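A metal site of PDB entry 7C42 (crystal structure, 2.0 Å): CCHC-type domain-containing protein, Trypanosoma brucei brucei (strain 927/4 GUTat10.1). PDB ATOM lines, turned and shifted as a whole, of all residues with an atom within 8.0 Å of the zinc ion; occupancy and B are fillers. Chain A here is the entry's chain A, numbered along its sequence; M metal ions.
N of Lys 296 lies close to SG of Cys 294, 3.4 Å away. SG of Cys 294 lies close to N of Lys 297, at 3.6 Å. SG of Cys 281 sits close to N of Phe 283 (3.5 Å). The backbone NH of Cys 281 sits at hydrogen-bond distance from the backbone carbonyl oxygen of Glu 286. The side-chain sulfur of Cys 284 sits close to the backbone NH of Glu 286 (3.7 Å).
Along chain A the residues within 4 Å of the zinc ion span positions 281 to 294. The nearest printed residue that does not touch the zinc ion is Phe 283 (4.9 Å).
The zinc ion is bound by a ring nitrogen (NE2) of His 289, the side-chain sulfur of Cys 294, the side-chain sulfur of Cys 281 and the side-chain sulfur of Cys 284. The zinc ion has four donor atoms within binding distance.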
ATOM      1  N   LYS A 280      -9.590  13.827 -32.674  1.00  0.00           N
ATOM      2  CA  LYS A 280     -11.009  14.000 -32.951  1.00  0.00           C
ATOM      3  C   LYS A 280     -11.601  12.619 -33.219  1.00  0.00           C
ATOM      4  O   LYS A 280     -11.141  11.915 -34.124  1.00  0.00           O
ATOM      5  CB  LYS A 280     -11.232  14.941 -34.134  1.00  0.00           C
ATOM      6  CG  LYS A 280     -12.696  15.295 -34.405  1.00  0.00           C
ATOM      7  CD  LYS A 280     -12.836  16.021 -35.745  1.00  0.00           C
ATOM      8  CE  LYS A 280     -14.288  16.186 -36.134  1.00  0.00           C
ATOM      9  NZ  LYS A 280     -15.038  16.958 -35.114  1.00  0.00           N
ATOM     10  N   CYS A 281     -12.606  12.237 -32.438  1.00  0.00           N
ATOM     11  CA  CYS A 281     -13.106  10.874 -32.459  1.00  0.00           C
ATOM     12  C   CYS A 281     -13.852  10.592 -33.760  1.00  0.00           C
ATOM     13  O   CYS A 281     -14.845  11.238 -34.081  1.00  0.00           O
ATOM     14  CB  CYS A 281     -14.021  10.652 -31.254  1.00  0.00           C
ATOM     15  SG  CYS A 281     -14.705   9.003 -31.158  1.00  0.00           S
ATOM     16  N   SER A 282     -13.382   9.592 -34.515  1.00  0.00           N
ATOM     17  CA  SER A 282     -14.030   9.257 -35.762  1.00  0.00           C
ATOM     18  C   SER A 282     -15.428   8.678 -35.562  1.00  0.00           C
ATOM     19  O   SER A 282     -16.210   8.638 -36.523  1.00  0.00           O
ATOM     20  CB  SER A 282     -13.174   8.272 -36.549  1.00  0.00           C
ATOM     21  OG  SER A 282     -12.886   7.127 -35.778  1.00  0.00           O
ATOM     22  N   PHE A 283     -15.766   8.238 -34.357  1.00  0.00           N
ATOM     23  CA  PHE A 283     -17.064   7.598 -34.136  1.00  0.00           C
ATOM     24  C   PHE A 283     -18.125   8.553 -33.604  1.00  0.00           C
ATOM     25  O   PHE A 283     -19.273   8.492 -34.040  1.00  0.00           O
ATOM     26  CB  PHE A 283     -16.924   6.412 -33.169  1.00  0.00           C
ATOM     27  CG  PHE A 283     -18.151   5.552 -33.095  1.00  0.00           C
ATOM     28  CD1 PHE A 283     -18.495   4.722 -34.159  1.00  0.00           C
ATOM     29  CD2 PHE A 283     -18.977   5.593 -31.974  1.00  0.00           C
ATOM     30  CE1 PHE A 283     -19.646   3.935 -34.094  1.00  0.00           C
ATOM     31  CE2 PHE A 283     -20.115   4.803 -31.914  1.00  0.00           C
ATOM     32  CZ  PHE A 283     -20.450   3.974 -32.974  1.00  0.00           C
ATOM     33  N   CYS A 284     -17.770   9.448 -32.664  1.00  0.00           N
ATOM     34  CA  CYS A 284     -18.741  10.391 -32.108  1.00  0.00           C
ATOM     35  C   CYS A 284     -18.426  11.836 -32.427  1.00  0.00           C
ATOM     36  O   CYS A 284     -19.252  12.709 -32.153  1.00  0.00           O
ATOM     37  CB  CYS A 284     -18.863  10.208 -30.582  1.00  0.00           C
ATOM     38  SG  CYS A 284     -17.426  10.851 -29.651  1.00  0.00           S
ATOM     39  N   GLY A 285     -17.268  12.120 -33.013  1.00  0.00           N
ATOM     40  CA  GLY A 285     -16.946  13.454 -33.476  1.00  0.00           C
ATOM     41  C   GLY A 285     -16.376  14.391 -32.436  1.00  0.00           C
ATOM     42  O   GLY A 285     -15.974  15.503 -32.799  1.00  0.00           O
ATOM     43  N   GLU A 286     -16.322  13.986 -31.171  1.00  0.00           N
ATOM     44  CA  GLU A 286     -15.835  14.868 -30.110  1.00  0.00           C
ATOM     45  C   GLU A 286     -14.336  15.101 -30.238  1.00  0.00           C
ATOM     46  O   GLU A 286     -13.568  14.181 -30.536  1.00  0.00           O
ATOM     47  CB  GLU A 286     -16.155  14.294 -28.738  1.00  0.00           C
ATOM     48  CG  GLU A 286     -17.652  14.097 -28.454  1.00  0.00           C
ATOM     49  CD  GLU A 286     -17.932  13.359 -27.139  1.00  0.00           C
ATOM     50  OE1 GLU A 286     -17.005  13.227 -26.319  1.00  0.00           O
ATOM     51  OE2 GLU A 286     -19.088  12.906 -26.929  1.00  0.00           O
ATOM     52  N   VAL A 287     -13.909  16.345 -30.013  1.00  0.00           N
ATOM     53  CA  VAL A 287     -12.485  16.637 -29.896  1.00  0.00           C
ATOM     54  C   VAL A 287     -11.996  16.144 -28.537  1.00  0.00           C
ATOM     55  O   VAL A 287     -12.703  16.238 -27.533  1.00  0.00           O
ATOM     56  CB  VAL A 287     -12.216  18.139 -30.083  1.00  0.00           C
ATOM     57  CG1 VAL A 287     -10.732  18.441 -29.868  1.00  0.00           C
ATOM     58  CG2 VAL A 287     -12.665  18.589 -31.472  1.00  0.00           C
ATOM     59  N   GLY A 288     -10.800  15.556 -28.513  1.00  0.00           N
ATOM     60  CA  GLY A 288     -10.145  15.177 -27.287  1.00  0.00           C
ATOM     61  C   GLY A 288      -9.878  13.699 -27.105  1.00  0.00           C
ATOM     62  O   GLY A 288      -9.049  13.342 -26.256  1.00  0.00           O
ATOM     63  N   HIS A 289     -10.545  12.807 -27.863  1.00  0.00           N
ATOM     64  CA  HIS A 289     -10.269  11.379 -27.734  1.00  0.00           C
ATOM     65  C   HIS A 289     -10.372  10.699 -29.095  1.00  0.00           C
ATOM     66  O   HIS A 289     -10.996  11.220 -30.028  1.00  0.00           O
ATOM     67  CB  HIS A 289     -11.199  10.707 -26.713  1.00  0.00           C
ATOM     68  CG  HIS A 289     -12.626  10.618 -27.135  1.00  0.00           C
ATOM     69  ND1 HIS A 289     -13.551  11.605 -26.851  1.00  0.00           N
ATOM     70  CD2 HIS A 289     -13.311   9.651 -27.805  1.00  0.00           C
ATOM     71  CE1 HIS A 289     -14.726  11.258 -27.336  1.00  0.00           C
ATOM     72  NE2 HIS A 289     -14.618  10.072 -27.917  1.00  0.00           N
ATOM     73  N   THR A 290      -9.727   9.546 -29.205  1.00  0.00           N
ATOM     74  CA  THR A 290      -9.709   8.766 -30.435  1.00  0.00           C
ATOM     75  C   THR A 290     -10.773   7.674 -30.368  1.00  0.00           C
ATOM     76  O   THR A 290     -11.218   7.283 -29.281  1.00  0.00           O
ATOM     77  CB  THR A 290      -8.337   8.128 -30.638  1.00  0.00           C
ATOM     78  OG1 THR A 290      -8.108   7.178 -29.587  1.00  0.00           O
ATOM     79  CG2 THR A 290      -7.244   9.172 -30.610  1.00  0.00           C
ATOM     80  N   ALA A 291     -11.163   7.171 -31.530  1.00  0.00           N
ATOM     81  CA  ALA A 291     -12.210   6.145 -31.546  1.00  0.00           C
ATOM     82  C   ALA A 291     -11.822   4.921 -30.744  1.00  0.00           C
ATOM     83  O   ALA A 291     -12.682   4.288 -30.120  1.00  0.00           O
ATOM     84  CB  ALA A 291     -12.567   5.749 -32.975  1.00  0.00           C
ATOM     85  N   ARG A 292     -10.529   4.575 -30.722  1.00  0.00           N
ATOM     86  CA  ARG A 292     -10.064   3.433 -29.935  1.00  0.00           C
ATOM     87  C   ARG A 292     -10.393   3.601 -28.458  1.00  0.00           C
ATOM     88  O   ARG A 292     -10.633   2.605 -27.761  1.00  0.00           O
ATOM     89  CB  ARG A 292      -8.549   3.230 -30.127  1.00  0.00           C
ATOM     90  N   ASN A 293     -10.441   4.838 -27.982  1.00  0.00           N
ATOM     91  CA  ASN A 293     -10.722   5.123 -26.580  1.00  0.00           C
ATOM     92  C   ASN A 293     -12.145   5.647 -26.355  1.00  0.00           C
ATOM     93  O   ASN A 293     -12.447   6.139 -25.270  1.00  0.00           O
ATOM     94  CB  ASN A 293      -9.686   6.138 -26.043  1.00  0.00           C
ATOM     95  CG  ASN A 293      -8.268   5.566 -26.076  1.00  0.00           C
ATOM     96  OD1 ASN A 293      -8.058   4.437 -25.669  1.00  0.00           O
ATOM     97  ND2 ASN A 293      -7.320   6.333 -26.590  1.00  0.00           N
ATOM     98  N   CYS A 294     -13.038   5.519 -27.352  1.00  0.00           N
ATOM     99  CA  CYS A 294     -14.375   6.080 -27.236  1.00  0.00           C
ATOM    100  C   CYS A 294     -15.289   5.134 -26.455  1.00  0.00           C
ATOM    101  O   CYS A 294     -15.527   4.008 -26.880  1.00  0.00           O
ATOM    102  CB  CYS A 294     -14.966   6.359 -28.624  1.00  0.00           C
ATOM    103  SG  CYS A 294     -16.631   7.131 -28.602  1.00  0.00           S
ATOM    104  N   PHE A 295     -15.813   5.627 -25.322  1.00  0.00           N
ATOM    105  CA  PHE A 295     -16.782   4.860 -24.539  1.00  0.00           C
ATOM    106  C   PHE A 295     -18.062   4.555 -25.327  1.00  0.00           C
ATOM    107  O   PHE A 295     -18.716   3.531 -25.086  1.00  0.00           O
ATOM    108  CB  PHE A 295     -17.140   5.616 -23.250  1.00  0.00           C
ATOM    109  CG  PHE A 295     -16.001   5.753 -22.283  1.00  0.00           C
ATOM    110  CD1 PHE A 295     -15.545   4.658 -21.555  1.00  0.00           C
ATOM    111  CD2 PHE A 295     -15.383   6.982 -22.073  1.00  0.00           C
ATOM    112  CE1 PHE A 295     -14.488   4.780 -20.655  1.00  0.00           C
ATOM    113  CE2 PHE A 295     -14.328   7.117 -21.171  1.00  0.00           C
ATOM    114  CZ  PHE A 295     -13.884   6.009 -20.465  1.00  0.00           C
ATOM    115  N   LYS A 296     -18.437   5.429 -26.261  1.00  0.00           N
ATOM    116  CA  LYS A 296     -19.653   5.184 -27.045  1.00  0.00           C
ATOM    117  C   LYS A 296     -19.453   4.035 -28.024  1.00  0.00           C
ATOM    118  O   LYS A 296     -20.343   3.196 -28.185  1.00  0.00           O
ATOM    119  CB  LYS A 296     -20.074   6.460 -27.781  1.00  0.00           C
ATOM    120  CG  LYS A 296     -20.360   7.641 -26.850  1.00  0.00           C
ATOM    121  CD  LYS A 296     -20.595   8.930 -27.633  1.00  0.00           C
ATOM    122  CE  LYS A 296     -21.542   9.881 -26.907  1.00  0.00           C
ATOM    123  NZ  LYS A 296     -21.963  11.015 -27.782  1.00  0.00           N
ATOM    124  N   LYS A 297     -18.292   3.979 -28.688  1.00  0.00           N
ATOM    125  CA  LYS A 297     -18.017   2.880 -29.599  1.00  0.00           C
ATOM    126  C   LYS A 297     -17.695   1.600 -28.856  1.00  0.00           C
ATOM    127  O   LYS A 297     -17.958   0.510 -29.378  1.00  0.00           O
ATOM    128  CB  LYS A 297     -16.851   3.251 -30.525  1.00  0.00           C
ATOM    129  CG  LYS A 297     -16.580   2.257 -31.631  1.00  0.00           C
ATOM    130  CD  LYS A 297     -15.438   2.712 -32.532  1.00  0.00           C
ATOM    131  CE  LYS A 297     -15.276   1.775 -33.724  1.00  0.00           C
ATOM    132  NZ  LYS A 297     -14.358   2.323 -34.737  1.00  0.00           N
ATOM    133  N   HIS A 298     -17.142   1.704 -27.648  1.00  0.00           N
ATOM    134  CA  HIS A 298     -16.598   0.569 -26.904  1.00  0.00           C
ATOM    135  C   HIS A 298     -17.166   0.586 -25.496  1.00  0.00           C
ATOM    136  O   HIS A 298     -16.474   0.971 -24.550  1.00  0.00           O
ATOM    137  CB  HIS A 298     -15.071   0.603 -26.857  1.00  0.00           C
ATOM    138  CG  HIS A 298     -14.419   0.704 -28.199  1.00  0.00           C
ATOM    139  ND1 HIS A 298     -14.435  -0.318 -29.117  1.00  0.00           N
ATOM    140  CD2 HIS A 298     -13.687   1.694 -28.763  1.00  0.00           C
ATOM    141  CE1 HIS A 298     -13.763   0.038 -30.189  1.00  0.00           C
ATOM    142  NE2 HIS A 298     -13.295   1.256 -30.005  1.00  0.00           N
HETATM  143 ZN    ZN M   1     -15.960   9.146 -29.274  1.00  0.00          ZN
